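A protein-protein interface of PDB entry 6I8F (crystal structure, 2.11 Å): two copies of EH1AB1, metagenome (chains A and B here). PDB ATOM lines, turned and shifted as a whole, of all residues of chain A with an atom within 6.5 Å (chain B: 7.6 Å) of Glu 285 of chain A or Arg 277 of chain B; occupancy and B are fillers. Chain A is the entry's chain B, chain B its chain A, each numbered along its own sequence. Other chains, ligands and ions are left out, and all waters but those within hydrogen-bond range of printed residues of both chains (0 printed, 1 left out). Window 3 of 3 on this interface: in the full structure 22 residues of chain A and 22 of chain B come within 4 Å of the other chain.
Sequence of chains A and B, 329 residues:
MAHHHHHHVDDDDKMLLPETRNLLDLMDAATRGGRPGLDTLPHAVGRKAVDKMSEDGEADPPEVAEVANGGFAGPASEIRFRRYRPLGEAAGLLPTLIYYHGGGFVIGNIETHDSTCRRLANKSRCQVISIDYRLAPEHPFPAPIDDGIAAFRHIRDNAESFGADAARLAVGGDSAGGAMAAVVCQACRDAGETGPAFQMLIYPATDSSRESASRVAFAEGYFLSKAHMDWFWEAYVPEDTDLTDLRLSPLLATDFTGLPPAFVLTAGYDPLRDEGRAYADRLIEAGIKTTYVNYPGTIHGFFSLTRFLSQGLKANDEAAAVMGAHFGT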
ATOM      1  N   ALA A 280      13.385  11.871  -1.108  1.00  0.00           N
ATOM      2  CA  ALA A 280      14.078  11.300   0.048  1.00  0.00           C
ATOM      3  C   ALA A 280      13.190  11.413   1.298  1.00  0.00           C
ATOM      4  O   ALA A 280      13.084  10.465   2.072  1.00  0.00           O
ATOM      5  CB  ALA A 280      15.407  11.980   0.257  1.00  0.00           C
ATOM      6  N   ASP A 281      12.560  12.574   1.492  1.00  0.00           N
ATOM      7  CA  ASP A 281      11.658  12.764   2.635  1.00  0.00           C
ATOM      8  C   ASP A 281      10.521  11.730   2.607  1.00  0.00           C
ATOM      9  O   ASP A 281      10.155  11.223   3.668  1.00  0.00           O
ATOM     10  CB  ASP A 281      11.053  14.167   2.706  1.00  0.00           C
ATOM     11  CG  ASP A 281      12.037  15.273   3.053  1.00  0.00           C
ATOM     12  OD1 ASP A 281      13.074  14.984   3.707  1.00  0.00           O
ATOM     13  OD2 ASP A 281      11.763  16.416   2.652  1.00  0.00           O
ATOM     14  N   ARG A 282       9.961  11.425   1.429  1.00  0.00           N
ATOM     15  CA  ARG A 282       8.860  10.437   1.358  1.00  0.00           C
ATOM     16  C   ARG A 282       9.390   9.039   1.719  1.00  0.00           C
ATOM     17  O   ARG A 282       8.695   8.260   2.394  1.00  0.00           O
ATOM     18  CB  ARG A 282       8.178  10.423  -0.015  1.00  0.00           C
ATOM     19  CG  ARG A 282       7.405  11.684  -0.390  1.00  0.00           C
ATOM     20  CD  ARG A 282       5.991  11.809   0.148  1.00  0.00           C
ATOM     21  NE  ARG A 282       5.204  10.576   0.163  1.00  0.00           N
ATOM     22  CZ  ARG A 282       4.252  10.228  -0.718  1.00  0.00           C
ATOM     23  NH1 ARG A 282       4.030  10.935  -1.815  1.00  0.00           N
ATOM     24  NH2 ARG A 282       3.519   9.150  -0.491  1.00  0.00           N
ATOM     25  N   LEU A 283      10.622   8.723   1.286  1.00  0.00           N
ATOM     26  CA  LEU A 283      11.239   7.437   1.590  1.00  0.00           C
ATOM     27  C   LEU A 283      11.484   7.326   3.098  1.00  0.00           C
ATOM     28  O   LEU A 283      11.151   6.316   3.718  1.00  0.00           O
ATOM     29  CB  LEU A 283      12.536   7.274   0.783  1.00  0.00           C
ATOM     30  CG  LEU A 283      12.355   7.089  -0.723  1.00  0.00           C
ATOM     31  CD1 LEU A 283      13.647   7.369  -1.485  1.00  0.00           C
ATOM     32  CD2 LEU A 283      11.847   5.688  -1.038  1.00  0.00           C
ATOM     33  N   ILE A 284      12.048   8.382   3.690  1.00  0.00           N
ATOM     34  CA  ILE A 284      12.391   8.397   5.111  1.00  0.00           C
ATOM     35  C   ILE A 284      11.111   8.152   5.919  1.00  0.00           C
ATOM     36  O   ILE A 284      11.071   7.286   6.791  1.00  0.00           O
ATOM     37  CB  ILE A 284      13.112   9.704   5.494  1.00  0.00           C
ATOM     38  CG1 ILE A 284      14.531   9.710   4.917  1.00  0.00           C
ATOM     39  CG2 ILE A 284      13.126   9.942   7.000  1.00  0.00           C
ATOM     40  CD1 ILE A 284      15.106  11.079   4.728  1.00  0.00           C
ATOM     41  N   GLU A 285      10.054   8.871   5.550  1.00  0.00           N
ATOM     42  CA  GLU A 285       8.825   8.870   6.312  1.00  0.00           C
ATOM     43  C   GLU A 285       8.083   7.534   6.147  1.00  0.00           C
ATOM     44  O   GLU A 285       7.360   7.155   7.034  1.00  0.00           O
ATOM     45  CB  GLU A 285       8.059  10.152   5.977  1.00  0.00           C
ATOM     46  CG  GLU A 285       8.679  11.345   6.706  1.00  0.00           C
ATOM     47  CD  GLU A 285       8.527  12.713   6.066  1.00  0.00           C
ATOM     48  OE1 GLU A 285       7.463  12.965   5.447  1.00  0.00           O
ATOM     49  OE2 GLU A 285       9.479  13.528   6.196  1.00  0.00           O
ATOM     50  N   ALA A 286       8.330   6.786   5.064  1.00  0.00           N
ATOM     51  CA  ALA A 286       7.754   5.458   4.891  1.00  0.00           C
ATOM     52  C   ALA A 286       8.588   4.378   5.607  1.00  0.00           C
ATOM     53  O   ALA A 286       8.260   3.211   5.520  1.00  0.00           O
ATOM     54  CB  ALA A 286       7.627   5.148   3.419  1.00  0.00           C
ATOM     55  N   GLY A 287       9.669   4.772   6.289  1.00  0.00           N
ATOM     56  CA  GLY A 287      10.525   3.863   7.039  1.00  0.00           C
ATOM     57  C   GLY A 287      11.494   3.095   6.156  1.00  0.00           C
ATOM     58  O   GLY A 287      11.888   1.977   6.494  1.00  0.00           O
ATOM     59  N   ILE A 288      11.887   3.690   5.025  1.00  0.00           N
ATOM     60  CA  ILE A 288      12.910   3.128   4.147  1.00  0.00           C
ATOM     61  C   ILE A 288      14.269   3.678   4.593  1.00  0.00           C
ATOM     62  O   ILE A 288      14.389   4.864   4.853  1.00  0.00           O
ATOM     63  CB  ILE A 288      12.636   3.474   2.665  1.00  0.00           C
ATOM     64  CG1 ILE A 288      11.239   3.053   2.193  1.00  0.00           C
ATOM     65  CG2 ILE A 288      13.728   2.902   1.776  1.00  0.00           C
ATOM     66  CD1 ILE A 288      10.892   1.606   2.468  1.00  0.00           C
ATOM     67  N   THR A 290      17.275   5.463   4.061  1.00  0.00           N
ATOM     68  CA  THR A 290      17.480   6.489   3.076  1.00  0.00           C
ATOM     69  C   THR A 290      18.634   7.400   3.505  1.00  0.00           C
ATOM     70  O   THR A 290      18.635   7.919   4.613  1.00  0.00           O
ATOM     71  CB  THR A 290      16.219   7.341   2.881  1.00  0.00           C
ATOM     72  OG1 THR A 290      15.114   6.474   2.623  1.00  0.00           O
ATOM     73  CG2 THR A 290      16.341   8.338   1.752  1.00  0.00           C
ATOM     74  N   PRO B 204      23.131  11.956  17.583  1.00  0.00           N
ATOM     75  CA  PRO B 204      23.474  12.923  18.622  1.00  0.00           C
ATOM     76  C   PRO B 204      22.242  13.367  19.423  1.00  0.00           C
ATOM     77  O   PRO B 204      21.137  13.366  18.885  1.00  0.00           O
ATOM     78  CB  PRO B 204      24.032  14.110  17.818  1.00  0.00           C
ATOM     79  CG  PRO B 204      23.301  14.029  16.488  1.00  0.00           C
ATOM     80  CD  PRO B 204      23.147  12.544  16.234  1.00  0.00           C
ATOM     81  N   THR B 206      20.827  16.783  20.676  1.00  0.00           N
ATOM     82  CA  THR B 206      21.058  18.144  20.167  1.00  0.00           C
ATOM     83  C   THR B 206      20.197  19.193  20.878  1.00  0.00           C
ATOM     84  O   THR B 206      20.396  20.389  20.653  1.00  0.00           O
ATOM     85  CB  THR B 206      20.819  18.227  18.656  1.00  0.00           C
ATOM     86  OG1 THR B 206      19.432  17.990  18.396  1.00  0.00           O
ATOM     87  CG2 THR B 206      21.699  17.267  17.881  1.00  0.00           C
ATOM     88  N   LEU B 251      21.219  22.469  18.825  1.00  0.00           N
ATOM     89  CA  LEU B 251      20.133  22.683  17.870  1.00  0.00           C
ATOM     90  C   LEU B 251      19.618  24.133  17.912  1.00  0.00           C
ATOM     91  O   LEU B 251      19.084  24.619  16.907  1.00  0.00           O
ATOM     92  CB  LEU B 251      18.987  21.708  18.150  1.00  0.00           C
ATOM     93  CG  LEU B 251      17.809  21.760  17.172  1.00  0.00           C
ATOM     94  CD1 LEU B 251      18.262  21.480  15.745  1.00  0.00           C
ATOM     95  CD2 LEU B 251      16.725  20.787  17.584  1.00  0.00           C
ATOM     96  N   VAL B 264      25.039  12.976   9.397  1.00  0.00           N
ATOM     97  CA  VAL B 264      24.130  12.883  10.550  1.00  0.00           C
ATOM     98  C   VAL B 264      23.306  11.598  10.397  1.00  0.00           C
ATOM     99  O   VAL B 264      22.622  11.402   9.387  1.00  0.00           O
ATOM    100  CB  VAL B 264      23.228  14.128  10.666  1.00  0.00           C
ATOM    101  CG1 VAL B 264      22.365  14.065  11.913  1.00  0.00           C
ATOM    102  CG2 VAL B 264      24.020  15.429  10.639  1.00  0.00           C
ATOM    103  N   LEU B 265      23.410  10.713  11.388  1.00  0.00           N
ATOM    104  CA  LEU B 265      22.738   9.442  11.364  1.00  0.00           C
ATOM    105  C   LEU B 265      21.723   9.400  12.511  1.00  0.00           C
ATOM    106  O   LEU B 265      22.062   9.779  13.640  1.00  0.00           O
ATOM    107  CB  LEU B 265      23.774   8.321  11.491  1.00  0.00           C
ATOM    108  CG  LEU B 265      23.220   6.896  11.443  1.00  0.00           C
ATOM    109  CD1 LEU B 265      24.234   5.942  10.839  1.00  0.00           C
ATOM    110  CD2 LEU B 265      22.817   6.412  12.828  1.00  0.00           C
ATOM    111  N   THR B 266      20.495   8.953  12.204  1.00  0.00           N
ATOM    112  CA  THR B 266      19.509   8.646  13.228  1.00  0.00           C
ATOM    113  C   THR B 266      19.111   7.168  13.170  1.00  0.00           C
ATOM    114  O   THR B 266      19.135   6.516  12.118  1.00  0.00           O
ATOM    115  CB  THR B 266      18.270   9.548  13.135  1.00  0.00           C
ATOM    116  OG1 THR B 266      17.693   9.382  11.840  1.00  0.00           O
ATOM    117  CG2 THR B 266      18.586  11.004  13.406  1.00  0.00           C
ATOM    118  N   LEU B 272      15.899  10.264  20.401  1.00  0.00           N
ATOM    119  CA  LEU B 272      16.740  11.365  19.894  1.00  0.00           C
ATOM    120  C   LEU B 272      16.633  11.503  18.365  1.00  0.00           C
ATOM    121  O   LEU B 272      17.245  12.404  17.799  1.00  0.00           O
ATOM    122  CB  LEU B 272      18.204  11.129  20.285  1.00  0.00           C
ATOM    123  CG  LEU B 272      18.542  11.121  21.776  1.00  0.00           C
ATOM    124  CD1 LEU B 272      20.049  11.121  21.964  1.00  0.00           C
ATOM    125  CD2 LEU B 272      17.932  12.301  22.506  1.00  0.00           C
ATOM    126  N   ARG B 273      15.859  10.624  17.712  1.00  0.00           N
ATOM    127  CA  ARG B 273      15.718  10.607  16.258  1.00  0.00           C
ATOM    128  C   ARG B 273      15.331  11.997  15.728  1.00  0.00           C
ATOM    129  O   ARG B 273      16.003  12.509  14.820  1.00  0.00           O
ATOM    130  CB  ARG B 273      14.687   9.550  15.838  1.00  0.00           C
ATOM    131  CG  ARG B 273      14.579   9.332  14.336  1.00  0.00           C
ATOM    132  CD  ARG B 273      13.359   8.488  13.990  1.00  0.00           C
ATOM    133  NE  ARG B 273      12.133   9.123  14.465  1.00  0.00           N
ATOM    134  CZ  ARG B 273      10.918   8.592  14.395  1.00  0.00           C
ATOM    135  NH1 ARG B 273      10.748   7.361  13.948  1.00  0.00           N
ATOM    136  NH2 ARG B 273       9.870   9.314  14.746  1.00  0.00           N
ATOM    137  N   ASP B 274      14.262  12.602  16.278  1.00  0.00           N
ATOM    138  CA  ASP B 274      13.692  13.835  15.703  1.00  0.00           C
ATOM    139  C   ASP B 274      14.702  14.989  15.792  1.00  0.00           C
ATOM    140  O   ASP B 274      14.868  15.746  14.850  1.00  0.00           O
ATOM    141  CB  ASP B 274      12.354  14.213  16.354  1.00  0.00           C
ATOM    142  CG  ASP B 274      11.201  13.270  16.032  1.00  0.00           C
ATOM    143  OD1 ASP B 274      11.402  12.334  15.220  1.00  0.00           O
ATOM    144  OD2 ASP B 274      10.099  13.484  16.592  1.00  0.00           O
ATOM    145  N   GLU B 275      15.379  15.132  16.927  1.00  0.00           N
ATOM    146  CA  GLU B 275      16.274  16.266  17.121  1.00  0.00           C
ATOM    147  C   GLU B 275      17.574  16.051  16.320  1.00  0.00           C
ATOM    148  O   GLU B 275      18.247  17.021  15.952  1.00  0.00           O
ATOM    149  CB  GLU B 275      16.475  16.511  18.616  1.00  0.00           C
ATOM    150  CG  GLU B 275      17.417  15.545  19.308  1.00  0.00           C
ATOM    151  CD  GLU B 275      17.238  15.531  20.822  1.00  0.00           C
ATOM    152  OE1 GLU B 275      16.096  15.314  21.267  1.00  0.00           O
ATOM    153  OE2 GLU B 275      18.228  15.746  21.547  1.00  0.00           O
ATOM    154  N   GLY B 276      17.928  14.788  16.043  1.00  0.00           N
ATOM    155  CA  GLY B 276      19.042  14.497  15.139  1.00  0.00           C
ATOM    156  C   GLY B 276      18.726  14.966  13.729  1.00  0.00           C
ATOM    157  O   GLY B 276      19.507  15.697  13.092  1.00  0.00           O
ATOM    158  N   ARG B 277      17.544  14.577  13.254  1.00  0.00           N
ATOM    159  CA  ARG B 277      17.101  14.949  11.926  1.00  0.00           C
ATOM    160  C   ARG B 277      16.965  16.475  11.836  1.00  0.00           C
ATOM    161  O   ARG B 277      17.416  17.097  10.859  1.00  0.00           O
ATOM    162  CB  ARG B 277      15.780  14.261  11.575  1.00  0.00           C
ATOM    163  CG  ARG B 277      15.400  14.440  10.116  1.00  0.00           C
ATOM    164  CD  ARG B 277      14.137  13.686   9.767  1.00  0.00           C
ATOM    165  NE  ARG B 277      13.833  13.878   8.360  1.00  0.00           N
ATOM    166  CZ  ARG B 277      12.680  13.576   7.792  1.00  0.00           C
ATOM    167  NH1 ARG B 277      11.723  12.999   8.508  1.00  0.00           N
ATOM    168  NH2 ARG B 277      12.486  13.884   6.519  1.00  0.00           N
ATOM    169  N   ALA B 278      16.368  17.075  12.871  1.00  0.00           N
ATOM    170  CA  ALA B 278      16.232  18.534  12.957  1.00  0.00           C
ATOM    171  C   ALA B 278      17.588  19.215  12.759  1.00  0.00           C
ATOM    172  O   ALA B 278      17.675  20.228  12.069  1.00  0.00           O
ATOM    173  CB  ALA B 278      15.613  18.924  14.280  1.00  0.00           C
ATOM    174  N   TYR B 279      18.641  18.669  13.380  1.00  0.00           N
ATOM    175  CA  TYR B 279      20.002  19.237  13.277  1.00  0.00           C
ATOM    176  C   TYR B 279      20.494  19.202  11.816  1.00  0.00           C
ATOM    177  O   TYR B 279      21.037  20.201  11.288  1.00  0.00           O
ATOM    178  CB  TYR B 279      20.956  18.526  14.240  1.00  0.00           C
ATOM    179  CG  TYR B 279      22.159  19.363  14.595  1.00  0.00           C
ATOM    180  CD1 TYR B 279      22.080  20.344  15.569  1.00  0.00           C
ATOM    181  CD2 TYR B 279      23.357  19.214  13.921  1.00  0.00           C
ATOM    182  CE1 TYR B 279      23.174  21.133  15.893  1.00  0.00           C
ATOM    183  CE2 TYR B 279      24.459  20.000  14.218  1.00  0.00           C
ATOM    184  CZ  TYR B 279      24.370  20.958  15.215  1.00  0.00           C
ATOM    185  OH  TYR B 279      25.447  21.745  15.507  1.00  0.00           O
ATOM    186  N   ALA B 280      20.286  18.071  11.146  1.00  0.00           N
ATOM    187  CA  ALA B 280      20.633  17.922   9.725  1.00  0.00           C
ATOM    188  C   ALA B 280      19.838  18.923   8.877  1.00  0.00           C
ATOM    189  O   ALA B 280      20.377  19.539   7.966  1.00  0.00           O
ATOM    190  CB  ALA B 280      20.384  16.501   9.276  1.00  0.00           C
ATOM    191  N   ASP B 281      18.546  19.075   9.190  1.00  0.00           N
ATOM    192  CA  ASP B 281      17.673  20.032   8.503  1.00  0.00           C
ATOM    193  C   ASP B 281      18.240  21.458   8.602  1.00  0.00           C
ATOM    194  O   ASP B 281      18.274  22.168   7.601  1.00  0.00           O
ATOM    195  CB  ASP B 281      16.242  19.985   9.048  1.00  0.00           C
ATOM    196  CG  ASP B 281      15.476  18.738   8.646  1.00  0.00           C
ATOM    197  OD1 ASP B 281      15.936  18.024   7.714  1.00  0.00           O
ATOM    198  OD2 ASP B 281      14.448  18.468   9.289  1.00  0.00           O
ATOM    199  N   ARG B 282      18.687  21.866   9.797  1.00  0.00           N
ATOM    200  CA  ARG B 282      19.240  23.211  10.005  1.00  0.00           C
ATOM    201  C   ARG B 282      20.545  23.360   9.218  1.00  0.00           C
ATOM    202  O   ARG B 282      20.794  24.433   8.606  1.00  0.00           O
ATOM    203  CB  ARG B 282      19.482  23.521  11.485  1.00  0.00           C
ATOM    204  CG  ARG B 282      18.238  23.507  12.369  1.00  0.00           C
ATOM    205  CD  ARG B 282      17.545  24.831  12.646  1.00  0.00           C
ATOM    206  NE  ARG B 282      18.372  26.029  12.569  1.00  0.00           N
ATOM    207  CZ  ARG B 282      18.650  26.861  13.577  1.00  0.00           C
ATOM    208  NH1 ARG B 282      18.384  26.538  14.833  1.00  0.00           N
ATOM    209  NH2 ARG B 282      19.212  28.028  13.318  1.00  0.00           N
ATOM    210  N   LEU B 283      21.372  22.301   9.226  1.00  0.00           N
ATOM    211  CA  LEU B 283      22.613  22.325   8.457  1.00  0.00           C
ATOM    212  C   LEU B 283      22.281  22.489   6.964  1.00  0.00           C
ATOM    213  O   LEU B 283      22.857  23.332   6.301  1.00  0.00           O
ATOM    214  CB  LEU B 283      23.432  21.057   8.723  1.00  0.00           C
ATOM    215  CG  LEU B 283      24.089  20.966  10.096  1.00  0.00           C
ATOM    216  CD1 LEU B 283      24.563  19.549  10.377  1.00  0.00           C
ATOM    217  CD2 LEU B 283      25.232  21.963  10.223  1.00  0.00           C
ATOM    218  N   ILE B 284      21.327  21.701   6.456  1.00  0.00           N
ATOM    219  CA  ILE B 284      20.995  21.716   5.018  1.00  0.00           C
ATOM    220  C   ILE B 284      20.500  23.113   4.620  1.00  0.00           C
ATOM    221  O   ILE B 284      20.946  23.690   3.629  1.00  0.00           O
ATOM    222  CB  ILE B 284      19.981  20.606   4.679  1.00  0.00           C
ATOM    223  CG1 ILE B 284      20.647  19.232   4.758  1.00  0.00           C
ATOM    224  CG2 ILE B 284      19.331  20.825   3.316  1.00  0.00           C
ATOM    225  CD1 ILE B 284      19.683  18.101   5.008  1.00  0.00           C
ATOM    226  N   GLU B 285      19.585  23.652   5.428  1.00  0.00           N
ATOM    227  CA  GLU B 285      18.929  24.915   5.145  1.00  0.00           C
ATOM    228  C   GLU B 285      19.930  26.081   5.191  1.00  0.00           C
ATOM    229  O   GLU B 285      19.733  27.062   4.487  1.00  0.00           O
ATOM    230  CB  GLU B 285      17.702  25.053   6.047  1.00  0.00           C
ATOM    231  CG  GLU B 285      16.507  24.298   5.483  1.00  0.00           C
ATOM    232  CD  GLU B 285      15.646  23.525   6.470  1.00  0.00           C
ATOM    233  OE1 GLU B 285      15.191  24.146   7.465  1.00  0.00           O
ATOM    234  OE2 GLU B 285      15.420  22.307   6.231  1.00  0.00           O
ATOM    235  N   THR B 290      25.578  18.360   3.672  1.00  0.00           N
ATOM    236  CA  THR B 290      25.076  17.544   4.740  1.00  0.00           C
ATOM    237  C   THR B 290      24.566  16.232   4.154  1.00  0.00           C
ATOM    238  O   THR B 290      23.746  16.248   3.251  1.00  0.00           O
ATOM    239  CB  THR B 290      23.956  18.251   5.509  1.00  0.00           C
ATOM    240  OG1 THR B 290      24.417  19.558   5.846  1.00  0.00           O
ATOM    241  CG2 THR B 290      23.526  17.497   6.750  1.00  0.00           C
ATOM    242  N   TYR B 292      22.434  13.060   5.427  1.00  0.00           N
ATOM    243  CA  TYR B 292      21.554  12.580   6.480  1.00  0.00           C
ATOM    244  C   TYR B 292      21.112  11.152   6.152  1.00  0.00           C
ATOM    245  O   TYR B 292      20.750  10.866   5.018  1.00  0.00           O
ATOM    246  CB  TYR B 292      20.311  13.463   6.639  1.00  0.00           C
ATOM    247  CG  TYR B 292      19.293  12.831   7.550  1.00  0.00           C
ATOM    248  CD1 TYR B 292      19.477  12.831   8.925  1.00  0.00           C
ATOM    249  CD2 TYR B 292      18.208  12.138   7.042  1.00  0.00           C
ATOM    250  CE1 TYR B 292      18.575  12.211   9.775  1.00  0.00           C
ATOM    251  CE2 TYR B 292      17.302  11.501   7.877  1.00  0.00           C
ATOM    252  CZ  TYR B 292      17.489  11.530   9.249  1.00  0.00           C
ATOM    253  OH  TYR B 292      16.595  10.912  10.078  1.00  0.00           O
ATOM    254  N   VAL B 293      21.127  10.272   7.154  1.00  0.00           N
ATOM    255  CA  VAL B 293      20.620   8.913   6.964  1.00  0.00           C
ATOM    256  C   VAL B 293      19.857   8.476   8.214  1.00  0.00           C
ATOM    257  O   VAL B 293      20.292   8.742   9.333  1.00  0.00           O
ATOM    258  CB  VAL B 293      21.734   7.905   6.619  1.00  0.00           C
ATOM    259  CG1 VAL B 293      22.834   7.867   7.666  1.00  0.00           C
ATOM    260  CG2 VAL B 293      21.156   6.513   6.398  1.00  0.00           C
ATOM    261  N   ASN B 294      18.732   7.786   7.975  1.00  0.00           N
ATOM    262  CA  ASN B 294      17.942   7.160   8.998  1.00  0.00           C
ATOM    263  C   ASN B 294      18.022   5.646   8.808  1.00  0.00           C
ATOM    264  O   ASN B 294      17.821   5.150   7.692  1.00  0.00           O
ATOM    265  CB  ASN B 294      16.487   7.638   9.000  1.00  0.00           C
ATOM    266  CG  ASN B 294      15.683   7.012  10.122  1.00  0.00           C
ATOM    267  OD1 ASN B 294      14.733   6.275   9.874  1.00  0.00           O
ATOM    268  ND2 ASN B 294      16.082   7.252  11.355  1.00  0.00           N
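The guanidinium group (NH2) of Arg 277 of chain B is in salt-bridge range of the side-chain carboxylate (OD1) of Asp 281 of chain A. OE2 of Glu 285 of chain A is in salt-bridge range of NH2 of Arg 277 of chain B (3.0 Å). N of Asn 294 of chain B sits at hydrogen-bond distance from O of Thr 290 of chain A.
The backbone NH (N) of Val 293 of chain B lies within hydrogen-bond range of the backbone carbonyl oxygen (O) of Val 264 of chain B (2.9 Å). OH of Tyr 292 of chain B sits at hydrogen-bond distance from OG1 of Thr 266 of chain B (2.6 Å). N of Thr 266 of chain B lies within hydrogen-bond range of O of Val 293 of chain B (2.9 Å). The side-chain hydroxyl of Thr 266 of chain B sits at hydrogen-bond distance from the side-chain amide nitrogen of Asn 294 of chain B (2.7 Å). O of Ile 288 of chain A lies within hydrogen-bond range of OG1 of Thr 290 of chain A.
Of the 10 printed residues of chain A, 4 touch a printed residue of chain B. Printed residues of chain A that touch a printed residue of chain B: Asp 281, Ile 284, Glu 285 and Thr 290. Hydrophobic or aromatic side chains of chain A within 4 Å of the printed part of chain B: Ile 284. Hydrophobic or aromatic side chains of chain B within 4 Å of the printed part of chain A: Tyr 292 and Val 293. Among the printed residues, 7 pairs touch across the chains.
7 positions are printed for both chains.
Arg 277 of chain B touches Ile 284 of chain A. Ile 284 of chain A touches Tyr 292 of chain B (CD1 to CE2, 3.9 Å). Thr 290 of chain A touches Tyr 292 of chain B. Thr 290 of chain A touches Val 293 of chain B (O to CA, 3.2 Å).
Of the printed residues of chain B, Asp 281 of chain A touches Arg 277 (3.1 Å). Of the printed residues of chain B, Ile 284 of chain A touches Arg 277 and Tyr 292. Glu 285 of chain A touches one residue of chain B. Gly 276 of chain B touches none of the printed residues of chain A. Arg 277 of chain B touches just these residues of chain A: Asp 281 (3.1 Å), Ile 284 (3.7 Å) and Glu 285 (3.0 Å). Of the printed residues of chain A, Tyr 292 of chain B touches Ile 284 (3.9 Å) and Thr 290 (3.6 Å). Of the printed residues of chain A, Val 293 of chain B touches Thr 290. Of the printed residues of chain A, Asn 294 of chain B touches Thr 290 (3.4 Å). The nearest residue of chain B that does not touch Glu 285 of chain A is Asn 294 of chain B (6.9 Å). The nearest printed residue of chain B that does not touch Asp 281 of chain A is Asp 281 of chain B (5.8 Å).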
